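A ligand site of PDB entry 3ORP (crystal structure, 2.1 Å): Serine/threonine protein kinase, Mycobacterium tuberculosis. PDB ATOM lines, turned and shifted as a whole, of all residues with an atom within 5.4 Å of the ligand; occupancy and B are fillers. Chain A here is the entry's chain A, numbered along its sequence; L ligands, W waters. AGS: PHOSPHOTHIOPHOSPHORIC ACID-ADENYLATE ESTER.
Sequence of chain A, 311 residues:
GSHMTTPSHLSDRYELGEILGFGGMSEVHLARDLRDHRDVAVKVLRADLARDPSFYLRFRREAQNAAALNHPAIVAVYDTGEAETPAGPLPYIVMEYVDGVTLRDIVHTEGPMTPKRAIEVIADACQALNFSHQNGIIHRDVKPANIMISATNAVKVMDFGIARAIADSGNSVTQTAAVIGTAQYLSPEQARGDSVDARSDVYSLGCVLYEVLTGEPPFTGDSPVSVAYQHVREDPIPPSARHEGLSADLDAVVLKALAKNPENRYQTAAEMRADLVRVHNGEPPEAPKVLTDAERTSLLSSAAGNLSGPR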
ATOM      1  N   LEU A  20     -14.660  13.564 -11.627  1.00  0.00           N
ATOM      2  CA  LEU A  20     -15.061  13.161 -10.282  1.00  0.00           C
ATOM      3  C   LEU A  20     -14.097  13.678  -9.219  1.00  0.00           C
ATOM      4  O   LEU A  20     -14.505  13.993  -8.097  1.00  0.00           O
ATOM      5  CB  LEU A  20     -15.114  11.636 -10.234  1.00  0.00           C
ATOM      6  CG  LEU A  20     -16.120  11.028 -11.214  1.00  0.00           C
ATOM      7  CD1 LEU A  20     -15.938   9.518 -11.361  1.00  0.00           C
ATOM      8  CD2 LEU A  20     -17.560  11.341 -10.780  1.00  0.00           C
ATOM      9  N   GLY A  21     -12.809  13.773  -9.580  1.00  0.00           N
ATOM     10  CA  GLY A  21     -11.815  14.061  -8.563  1.00  0.00           C
ATOM     11  C   GLY A  21     -10.429  14.206  -9.109  1.00  0.00           C
ATOM     12  O   GLY A  21     -10.187  14.017 -10.306  1.00  0.00           O
ATOM     13  N   PHE A  22      -9.522  14.604  -8.228  1.00  0.00           N
ATOM     14  CA  PHE A  22      -8.111  14.746  -8.567  1.00  0.00           C
ATOM     15  C   PHE A  22      -7.292  14.446  -7.330  1.00  0.00           C
ATOM     16  O   PHE A  22      -7.818  14.461  -6.188  1.00  0.00           O
ATOM     17  CB  PHE A  22      -7.791  16.164  -9.095  1.00  0.00           C
ATOM     18  CG  PHE A  22      -7.855  17.227  -8.022  1.00  0.00           C
ATOM     19  CD1 PHE A  22      -6.727  17.574  -7.287  1.00  0.00           C
ATOM     20  CD2 PHE A  22      -9.043  17.887  -7.757  1.00  0.00           C
ATOM     21  CE1 PHE A  22      -6.774  18.554  -6.322  1.00  0.00           C
ATOM     22  CE2 PHE A  22      -9.100  18.858  -6.792  1.00  0.00           C
ATOM     23  CZ  PHE A  22      -7.961  19.191  -6.065  1.00  0.00           C
ATOM     24  N   GLY A  23      -6.017  14.152  -7.547  1.00  0.00           N
ATOM     25  CA  GLY A  23      -5.050  13.976  -6.480  1.00  0.00           C
ATOM     26  C   GLY A  23      -3.759  14.646  -6.902  1.00  0.00           C
ATOM     27  O   GLY A  23      -3.748  15.490  -7.801  1.00  0.00           O
ATOM     28  N   GLY A  24      -2.656  14.263  -6.269  1.00  0.00           N
ATOM     29  CA  GLY A  24      -1.362  14.844  -6.623  1.00  0.00           C
ATOM     30  C   GLY A  24      -0.851  14.452  -7.998  1.00  0.00           C
ATOM     31  O   GLY A  24       0.007  15.111  -8.518  1.00  0.00           O
ATOM     32  N   MET A  25      -1.398  13.396  -8.594  1.00  0.00           N
ATOM     33  CA  MET A  25      -0.894  12.843  -9.855  1.00  0.00           C
ATOM     34  C   MET A  25      -1.953  12.727 -10.959  1.00  0.00           C
ATOM     35  O   MET A  25      -1.629  12.791 -12.169  1.00  0.00           O
ATOM     36  CB  MET A  25      -0.348  11.461  -9.538  1.00  0.00           C
ATOM     37  CG  MET A  25       0.516  10.844 -10.591  1.00  0.00           C
ATOM     38  SD  MET A  25       1.202   9.280  -9.968  1.00  0.00           S
ATOM     39  CE  MET A  25       0.078   8.051 -10.383  1.00  0.00           C
ATOM     40  N   SER A  26      -3.228  12.600 -10.543  1.00  0.00           N
ATOM     41  CA  SER A  26      -4.291  12.138 -11.438  1.00  0.00           C
ATOM     42  C   SER A  26      -5.498  13.006 -11.447  1.00  0.00           C
ATOM     43  O   SER A  26      -5.808  13.725 -10.473  1.00  0.00           O
ATOM     44  CB  SER A  26      -4.776  10.735 -11.038  1.00  0.00           C
ATOM     45  OG  SER A  26      -3.689   9.805 -10.934  1.00  0.00           O
ATOM     46  N   VAL A  28      -9.542  12.090 -12.292  1.00  0.00           N
ATOM     47  CA  VAL A  28     -10.424  10.916 -12.403  1.00  0.00           C
ATOM     48  C   VAL A  28     -11.779  11.386 -12.954  1.00  0.00           C
ATOM     49  O   VAL A  28     -12.393  12.278 -12.421  1.00  0.00           O
ATOM     50  CB  VAL A  28     -10.568  10.147 -11.046  1.00  0.00           C
ATOM     51  CG1 VAL A  28     -11.423   8.886 -11.215  1.00  0.00           C
ATOM     52  CG2 VAL A  28      -9.186   9.791 -10.485  1.00  0.00           C
ATOM     53  N   ALA A  41     -14.726   4.552 -13.796  1.00  0.00           N
ATOM     54  CA  ALA A  41     -13.946   5.707 -13.404  1.00  0.00           C
ATOM     55  C   ALA A  41     -12.615   5.556 -14.110  1.00  0.00           C
ATOM     56  O   ALA A  41     -11.952   4.535 -13.989  1.00  0.00           O
ATOM     57  CB  ALA A  41     -13.765   5.756 -11.939  1.00  0.00           C
ATOM     58  N   LYS A  43      -8.855   6.951 -14.383  1.00  0.00           N
ATOM     59  CA  LYS A  43      -7.791   7.701 -13.778  1.00  0.00           C
ATOM     60  C   LYS A  43      -6.716   7.977 -14.832  1.00  0.00           C
ATOM     61  O   LYS A  43      -6.055   7.060 -15.375  1.00  0.00           O
ATOM     62  CB  LYS A  43      -7.222   6.952 -12.575  1.00  0.00           C
ATOM     63  CG  LYS A  43      -6.146   7.724 -11.859  1.00  0.00           C
ATOM     64  CD  LYS A  43      -5.604   6.998 -10.635  1.00  0.00           C
ATOM     65  CE  LYS A  43      -6.561   7.056  -9.452  1.00  0.00           C
ATOM     66  NZ  LYS A  43      -5.842   6.574  -8.234  1.00  0.00           N
ATOM     67  N   ARG A  58       6.360   8.293 -12.957  1.00  0.00           N
ATOM     68  CA  ARG A  58       5.664   7.852 -11.740  1.00  0.00           C
ATOM     69  C   ARG A  58       4.275   7.273 -12.029  1.00  0.00           C
ATOM     70  O   ARG A  58       3.919   6.245 -11.481  1.00  0.00           O
ATOM     71  CB  ARG A  58       5.484   9.002 -10.750  1.00  0.00           C
ATOM     72  CG  ARG A  58       6.697   9.314  -9.946  1.00  0.00           C
ATOM     73  CD  ARG A  58       6.309  10.282  -8.823  1.00  0.00           C
ATOM     74  NE  ARG A  58       5.229   9.723  -8.010  1.00  0.00           N
ATOM     75  CZ  ARG A  58       4.520  10.443  -7.129  1.00  0.00           C
ATOM     76  NH1 ARG A  58       4.796  11.744  -6.957  1.00  0.00           N
ATOM     77  NH2 ARG A  58       3.551   9.877  -6.425  1.00  0.00           N
ATOM     78  N   ALA A  63       0.554   4.425 -10.102  1.00  0.00           N
ATOM     79  CA  ALA A  63      -0.904   4.403 -10.345  1.00  0.00           C
ATOM     80  C   ALA A  63      -1.364   3.297 -11.272  1.00  0.00           C
ATOM     81  O   ALA A  63      -2.375   2.693 -10.992  1.00  0.00           O
ATOM     82  CB  ALA A  63      -1.390   5.715 -10.889  1.00  0.00           C
ATOM     83  N   VAL A  75     -12.271  -1.476  -4.729  1.00  0.00           N
ATOM     84  CA  VAL A  75     -12.465  -0.909  -6.064  1.00  0.00           C
ATOM     85  C   VAL A  75     -11.741  -1.788  -7.072  1.00  0.00           C
ATOM     86  O   VAL A  75     -10.500  -1.931  -7.040  1.00  0.00           O
ATOM     87  CB  VAL A  75     -11.972   0.560  -6.145  1.00  0.00           C
ATOM     88  CG1 VAL A  75     -12.003   1.077  -7.583  1.00  0.00           C
ATOM     89  CG2 VAL A  75     -12.779   1.469  -5.194  1.00  0.00           C
ATOM     90  N   MET A  95     -11.112   1.787 -13.814  1.00  0.00           N
ATOM     91  CA  MET A  95     -11.537   1.092 -12.618  1.00  0.00           C
ATOM     92  C   MET A  95     -13.053   1.184 -12.360  1.00  0.00           C
ATOM     93  O   MET A  95     -13.788   1.875 -13.091  1.00  0.00           O
ATOM     94  CB  MET A  95     -10.748   1.615 -11.411  1.00  0.00           C
ATOM     95  CG  MET A  95     -11.112   2.979 -10.995  1.00  0.00           C
ATOM     96  SD  MET A  95      -9.826   3.732  -9.962  1.00  0.00           S
ATOM     97  CE  MET A  95      -8.562   4.034 -11.198  1.00  0.00           C
ATOM     98  N   GLU A  96     -13.463   0.406 -11.356  1.00  0.00           N
ATOM     99  CA  GLU A  96     -14.856   0.422 -10.837  1.00  0.00           C
ATOM    100  C   GLU A  96     -15.219   1.843 -10.425  1.00  0.00           C
ATOM    101  O   GLU A  96     -14.502   2.461  -9.680  1.00  0.00           O
ATOM    102  CB  GLU A  96     -14.993  -0.527  -9.636  1.00  0.00           C
ATOM    103  CG  GLU A  96     -16.389  -0.553  -8.985  1.00  0.00           C
ATOM    104  CD  GLU A  96     -16.442  -1.440  -7.742  1.00  0.00           C
ATOM    105  OE1 GLU A  96     -17.431  -1.317  -6.979  1.00  0.00           O
ATOM    106  OE2 GLU A  96     -15.513  -2.256  -7.543  1.00  0.00           O
ATOM    107  N   TYR A  97     -16.343   2.312 -10.932  1.00  0.00           N
ATOM    108  CA  TYR A  97     -16.904   3.590 -10.581  1.00  0.00           C
ATOM    109  C   TYR A  97     -17.597   3.489  -9.209  1.00  0.00           C
ATOM    110  O   TYR A  97     -18.463   2.611  -8.977  1.00  0.00           O
ATOM    111  CB  TYR A  97     -17.874   4.069 -11.650  1.00  0.00           C
ATOM    112  CG  TYR A  97     -18.752   5.231 -11.252  1.00  0.00           C
ATOM    113  CD1 TYR A  97     -18.196   6.407 -10.715  1.00  0.00           C
ATOM    114  CD2 TYR A  97     -20.139   5.168 -11.409  1.00  0.00           C
ATOM    115  CE1 TYR A  97     -18.992   7.476 -10.328  1.00  0.00           C
ATOM    116  CE2 TYR A  97     -20.955   6.240 -11.032  1.00  0.00           C
ATOM    117  CZ  TYR A  97     -20.366   7.385 -10.490  1.00  0.00           C
ATOM    118  OH  TYR A  97     -21.151   8.455 -10.143  1.00  0.00           O
ATOM    119  N   VAL A  98     -17.188   4.374  -8.309  1.00  0.00           N
ATOM    120  CA  VAL A  98     -17.850   4.542  -7.034  1.00  0.00           C
ATOM    121  C   VAL A  98     -18.520   5.897  -7.061  1.00  0.00           C
ATOM    122  O   VAL A  98     -17.856   6.921  -7.194  1.00  0.00           O
ATOM    123  CB  VAL A  98     -16.858   4.474  -5.866  1.00  0.00           C
ATOM    124  CG1 VAL A  98     -17.577   4.700  -4.551  1.00  0.00           C
ATOM    125  CG2 VAL A  98     -16.121   3.115  -5.861  1.00  0.00           C
ATOM    126  N   ASP A  99     -19.832   5.911  -6.925  1.00  0.00           N
ATOM    127  CA  ASP A  99     -20.589   7.152  -6.731  1.00  0.00           C
ATOM    128  C   ASP A  99     -20.596   7.441  -5.250  1.00  0.00           C
ATOM    129  O   ASP A  99     -21.341   6.817  -4.536  1.00  0.00           O
ATOM    130  CB  ASP A  99     -22.030   6.979  -7.219  1.00  0.00           C
ATOM    131  CG  ASP A  99     -22.870   8.216  -7.070  1.00  0.00           C
ATOM    132  OD1 ASP A  99     -22.383   9.285  -6.678  1.00  0.00           O
ATOM    133  OD2 ASP A  99     -24.055   8.114  -7.373  1.00  0.00           O
ATOM    134  N   THR A 102     -14.654  10.229  -0.520  1.00  0.00           N
ATOM    135  CA  THR A 102     -13.590   9.682   0.315  1.00  0.00           C
ATOM    136  C   THR A 102     -13.766  10.108   1.778  1.00  0.00           C
ATOM    137  O   THR A 102     -14.387  11.145   2.073  1.00  0.00           O
ATOM    138  CB  THR A 102     -12.178  10.161  -0.083  1.00  0.00           C
ATOM    139  OG1 THR A 102     -12.030  11.556   0.246  1.00  0.00           O
ATOM    140  CG2 THR A 102     -11.916   9.913  -1.540  1.00  0.00           C
ATOM    141  N   ARG A 104     -11.453  11.316   3.528  1.00  0.00           N
ATOM    142  CA  ARG A 104     -10.817  12.645   3.620  1.00  0.00           C
ATOM    143  C   ARG A 104     -11.851  13.727   3.360  1.00  0.00           C
ATOM    144  O   ARG A 104     -11.916  14.730   4.062  1.00  0.00           O
ATOM    145  CB  ARG A 104      -9.641  12.773   2.639  1.00  0.00           C
ATOM    146  CG  ARG A 104      -9.045  14.173   2.505  1.00  0.00           C
ATOM    147  CD  ARG A 104      -7.761  14.181   1.712  1.00  0.00           C
ATOM    148  NE  ARG A 104      -8.036  13.972   0.301  1.00  0.00           N
ATOM    149  CZ  ARG A 104      -7.136  13.738  -0.657  1.00  0.00           C
ATOM    150  NH1 ARG A 104      -5.824  13.635  -0.405  1.00  0.00           N
ATOM    151  NH2 ARG A 104      -7.576  13.589  -1.906  1.00  0.00           N
ATOM    152  N   ASP A 105     -12.652  13.529   2.312  1.00  0.00           N
ATOM    153  CA  ASP A 105     -13.744  14.458   2.011  1.00  0.00           C
ATOM    154  C   ASP A 105     -14.718  14.549   3.186  1.00  0.00           C
ATOM    155  O   ASP A 105     -15.023  15.626   3.659  1.00  0.00           O
ATOM    156  CB  ASP A 105     -14.567  14.015   0.784  1.00  0.00           C
ATOM    157  CG  ASP A 105     -13.801  14.086  -0.521  1.00  0.00           C
ATOM    158  OD1 ASP A 105     -12.888  14.951  -0.653  1.00  0.00           O
ATOM    159  OD2 ASP A 105     -14.137  13.257  -1.440  1.00  0.00           O
ATOM    160  N   ASP A 141      -0.551   1.885   1.370  1.00  0.00           N
ATOM    161  CA  ASP A 141      -0.928   3.314   1.475  1.00  0.00           C
ATOM    162  C   ASP A 141      -2.369   3.509   1.975  1.00  0.00           C
ATOM    163  O   ASP A 141      -3.195   4.206   1.333  1.00  0.00           O
ATOM    164  CB  ASP A 141      -0.719   4.011   0.119  1.00  0.00           C
ATOM    165  CG  ASP A 141      -0.557   5.508   0.244  1.00  0.00           C
ATOM    166  OD1 ASP A 141      -0.116   6.003   1.331  1.00  0.00           O
ATOM    167  OD2 ASP A 141      -0.867   6.195  -0.750  1.00  0.00           O
ATOM    168  N   LYS A 143      -5.007   5.242   3.799  1.00  0.00           N
ATOM    169  CA  LYS A 143      -5.175   6.635   4.170  1.00  0.00           C
ATOM    170  C   LYS A 143      -6.609   7.000   3.888  1.00  0.00           C
ATOM    171  O   LYS A 143      -7.285   6.340   3.128  1.00  0.00           O
ATOM    172  CB  LYS A 143      -4.212   7.559   3.408  1.00  0.00           C
ATOM    173  CG  LYS A 143      -4.400   7.592   1.880  1.00  0.00           C
ATOM    174  CD  LYS A 143      -3.202   8.267   1.190  1.00  0.00           C
ATOM    175  CE  LYS A 143      -3.430   8.385  -0.323  1.00  0.00           C
ATOM    176  NZ  LYS A 143      -2.409   9.263  -1.013  1.00  0.00           N
ATOM    177  N   ALA A 145      -7.963   9.154   1.891  1.00  0.00           N
ATOM    178  CA  ALA A 145      -8.238   9.383   0.465  1.00  0.00           C
ATOM    179  C   ALA A 145      -8.403   8.093  -0.313  1.00  0.00           C
ATOM    180  O   ALA A 145      -8.900   8.121  -1.428  1.00  0.00           O
ATOM    181  CB  ALA A 145      -7.119  10.163  -0.150  1.00  0.00           C
ATOM    182  N   ASN A 146      -7.949   6.982   0.247  1.00  0.00           N
ATOM    183  CA  ASN A 146      -8.035   5.686  -0.419  1.00  0.00           C
ATOM    184  C   ASN A 146      -9.221   4.867   0.029  1.00  0.00           C
ATOM    185  O   ASN A 146      -9.311   3.701  -0.355  1.00  0.00           O
ATOM    186  CB  ASN A 146      -6.698   4.936  -0.243  1.00  0.00           C
ATOM    187  CG  ASN A 146      -5.704   5.271  -1.321  1.00  0.00           C
ATOM    188  OD1 ASN A 146      -6.087   5.656  -2.413  1.00  0.00           O
ATOM    189  ND2 ASN A 146      -4.404   5.133  -1.018  1.00  0.00           N
ATOM    190  N   MET A 148     -13.478   5.104   0.090  1.00  0.00           N
ATOM    191  CA  MET A 148     -14.695   5.808  -0.294  1.00  0.00           C
ATOM    192  C   MET A 148     -15.904   5.173   0.382  1.00  0.00           C
ATOM    193  O   MET A 148     -15.913   3.966   0.638  1.00  0.00           O
ATOM    194  CB  MET A 148     -14.871   5.825  -1.799  1.00  0.00           C
ATOM    195  CG  MET A 148     -13.796   6.594  -2.568  1.00  0.00           C
ATOM    196  SD  MET A 148     -14.070   6.885  -4.332  1.00  0.00           S
ATOM    197  CE  MET A 148     -15.541   7.927  -4.288  1.00  0.00           C
ATOM    198  N   MET A 158      -9.415   1.426  -2.255  1.00  0.00           N
ATOM    199  CA  MET A 158      -8.725   1.397  -3.541  1.00  0.00           C
ATOM    200  C   MET A 158      -7.231   1.619  -3.496  1.00  0.00           C
ATOM    201  O   MET A 158      -6.688   2.036  -2.473  1.00  0.00           O
ATOM    202  CB  MET A 158      -9.348   2.442  -4.432  1.00  0.00           C
ATOM    203  CG  MET A 158      -9.169   3.836  -3.889  1.00  0.00           C
ATOM    204  SD  MET A 158     -10.467   4.895  -4.499  1.00  0.00           S
ATOM    205  CE  MET A 158      -9.698   6.506  -4.176  1.00  0.00           C
ATOM    206  N   ASP A 159      -6.576   1.288  -4.628  1.00  0.00           N
ATOM    207  CA  ASP A 159      -5.149   1.566  -4.908  1.00  0.00           C
ATOM    208  C   ASP A 159      -4.198   0.758  -4.041  1.00  0.00           C
ATOM    209  O   ASP A 159      -3.358   1.311  -3.298  1.00  0.00           O
ATOM    210  CB  ASP A 159      -4.857   3.074  -4.844  1.00  0.00           C
ATOM    211  CG  ASP A 159      -5.587   3.868  -5.929  1.00  0.00           C
ATOM    212  OD1 ASP A 159      -5.813   3.340  -7.017  1.00  0.00           O
ATOM    213  OD2 ASP A 159      -5.953   5.057  -5.718  1.00  0.00           O
ATOM    214  N   ILE A 180       4.149  11.600  -3.827  1.00  0.00           N
ATOM    215  CA  ILE A 180       2.988  12.375  -3.421  1.00  0.00           C
ATOM    216  C   ILE A 180       2.177  11.669  -2.355  1.00  0.00           C
ATOM    217  O   ILE A 180       1.731  10.516  -2.518  1.00  0.00           O
ATOM    218  CB  ILE A 180       1.957  12.569  -4.545  1.00  0.00           C
ATOM    219  CG1 ILE A 180       2.463  13.496  -5.631  1.00  0.00           C
ATOM    220  CG2 ILE A 180       0.663  13.179  -3.970  1.00  0.00           C
ATOM    221  CD1 ILE A 180       1.879  13.100  -6.951  1.00  0.00           C
HETATM  222  PG  AGS L   1      -2.369  10.456  -4.907  1.00  0.00           P
HETATM  223  S1G AGS L   1      -0.830  10.737  -5.719  1.00  0.00           S
HETATM  224  O2G AGS L   1      -2.863  11.876  -4.537  1.00  0.00           O
HETATM  225  O3G AGS L   1      -2.452   9.540  -3.682  1.00  0.00           O
HETATM  226  PB  AGS L   1      -3.990  10.244  -7.285  1.00  0.00           P
HETATM  227  O1B AGS L   1      -3.457  11.507  -7.849  1.00  0.00           O
HETATM  228  O2B AGS L   1      -3.816   9.126  -8.293  1.00  0.00           O
HETATM  229  O3B AGS L   1      -3.406   9.736  -5.880  1.00  0.00           O
HETATM  230  PA  AGS L   1      -6.605   9.629  -6.093  1.00  0.00           P
HETATM  231  O1A AGS L   1      -6.373   8.195  -6.255  1.00  0.00           O
HETATM  232  O2A AGS L   1      -6.598  10.195  -4.695  1.00  0.00           O
HETATM  233  O3A AGS L   1      -5.553  10.472  -6.962  1.00  0.00           O
HETATM  234  O5' AGS L   1      -7.967   9.942  -6.865  1.00  0.00           O
HETATM  235  C5' AGS L   1      -8.372  11.293  -6.894  1.00  0.00           C
HETATM  236  C4' AGS L   1      -9.852  11.429  -6.613  1.00  0.00           C
HETATM  237  O4' AGS L   1     -10.650  10.894  -7.678  1.00  0.00           O
HETATM  238  C3' AGS L   1     -10.336  10.747  -5.347  1.00  0.00           C
HETATM  239  O3' AGS L   1     -10.117  11.473  -4.166  1.00  0.00           O
HETATM  240  C2' AGS L   1     -11.803  10.626  -5.653  1.00  0.00           C
HETATM  241  O2' AGS L   1     -12.413  11.876  -5.462  1.00  0.00           O
HETATM  242  C1' AGS L   1     -11.841  10.315  -7.139  1.00  0.00           C
HETATM  243  N9  AGS L   1     -11.770   8.851  -7.362  1.00  0.00           N
HETATM  244  C8  AGS L   1     -10.663   8.026  -7.325  1.00  0.00           C
HETATM  245  N7  AGS L   1     -11.022   6.773  -7.615  1.00  0.00           N
HETATM  246  C5  AGS L   1     -12.347   6.768  -7.895  1.00  0.00           C
HETATM  247  C6  AGS L   1     -13.256   5.739  -8.224  1.00  0.00           C
HETATM  248  N6  AGS L   1     -12.844   4.483  -8.475  1.00  0.00           N
HETATM  249  N1  AGS L   1     -14.589   6.082  -8.412  1.00  0.00           N
HETATM  250  C2  AGS L   1     -15.011   7.367  -8.232  1.00  0.00           C
HETATM  251  N3  AGS L   1     -14.119   8.369  -7.878  1.00  0.00           N
HETATM  252  C4  AGS L   1     -12.824   8.067  -7.722  1.00  0.00           C
HETATM  253  O   HOH W   1      -5.106   8.790  -3.048  1.00  0.00           O
HETATM  254  O   HOH W   2     -15.280  10.754  -6.741  1.00  0.00           O
HETATM  255  O   HOH W   3      -5.205  12.024  -3.587  1.00  0.00           O
HETATM  256  O   HOH W   4      -2.875   6.338  -7.528  1.00  0.00           O
HETATM  257  O   HOH W   5       0.594   8.184  -3.182  1.00  0.00           O
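Water W3 lies within hydrogen-bond range of O2G of the ligand and NH2 of Arg 104. Water W1 lies within hydrogen-bond range of an oxygen (O2A) of the ligand (2.6 Å), the side-chain amide oxygen (OD1) of Asn 146 (3.3 Å) and the side-chain amino group (NZ) of Lys 143 (3.4 Å). Water W4 bridges O2B of the ligand (3.0 Å) and NZ of Lys 43 (3.1 Å). Water W5 lies within hydrogen-bond range of O of Ile 180 (2.7 Å), O3G of the ligand (3.4 Å) and OD2 of Asp 141 (3.5 Å).
The backbone NH of Met 158 sits at hydrogen-bond distance from the backbone carbonyl oxygen of Asn 146. OG1 of Thr 102 lies close to N of Arg 104 (3.3 Å). N of Met 95 sits at hydrogen-bond distance from O of Ala 41 (2.9 Å). The side-chain carboxylate of Asp 141 is in salt-bridge range of the side-chain amino group of Lys 143, 3.4 Å away. The backbone carbonyl oxygen of Val 28 lies within hydrogen-bond range of the backbone NH of Leu 20. The backbone NH of Val 28 is in hydrogen-bond range of the backbone carbonyl oxygen of Gly 21 (2.8 Å). The side-chain carboxylate of Asp 159 is in salt-bridge range of the side-chain amino group of Lys 43, 2.9 Å away. OD2 of Asp 159 sits close to OD1 of Asn 146 (3.4 Å).
The side-chain amino group (NZ) of Lys 43 is in salt-bridge range of an oxygen (O1A) of the ligand (2.6 Å). O2B of the ligand is in hydrogen-bond range of OG of Ser 26 (2.7 Å). N1 of the ligand is in hydrogen-bond range of N of Val 98 (3.1 Å). O2G of the ligand is in hydrogen-bond range of N of Gly 24. The backbone carbonyl oxygen of Glu 96 lies within hydrogen-bond range of a nitrogen (N6) of the ligand (2.9 Å). An oxygen (O1B) of the ligand lies within hydrogen-bond range of the backbone NH of Ser 26, 2.9 Å away. SD of Met 95 lies close to N6 of the ligand (3.4 Å). The backbone NH (N) of Met 25 lies within hydrogen-bond range of an oxygen (O1B) of the ligand (2.9 Å). The side-chain amino group (NZ) of Lys 143 lies within hydrogen-bond range of an oxygen (O3G) of the ligand (2.7 Å).
The side-chain sulfur of Met 158 sits close to a nitrogen (N7) of the ligand. The side-chain carboxylate (OD2) of Asp 159 lies close to an oxygen (O1A) of the ligand (3.2 Å). CD1 of Leu 20 touches C2 of the ligand, 3.9 Å away. CA of Gly 21 touches O4' of the ligand (3.5 Å). Phe 22 touches the ligand (O to C5', 3.3 Å). Gly 23 touches the ligand (CA to O1B, 3.2 Å). Val 28 touches the ligand. CB of Ala 41 touches N1 of the ligand, at 3.6 Å. Val 75 touches the ligand. Thr 102 touches the ligand. Met 148 touches the ligand. Ile 180 touches the ligand. Hydrophobic or aromatic side chains that line the ligand: Leu 20, Met 25, Val 28, Ala 41, Val 75, Met 95, Val 98, Met 148, Met 158 and Ile 180. Of the 29 residues printed, 20 come within 4 Å of the ligand.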
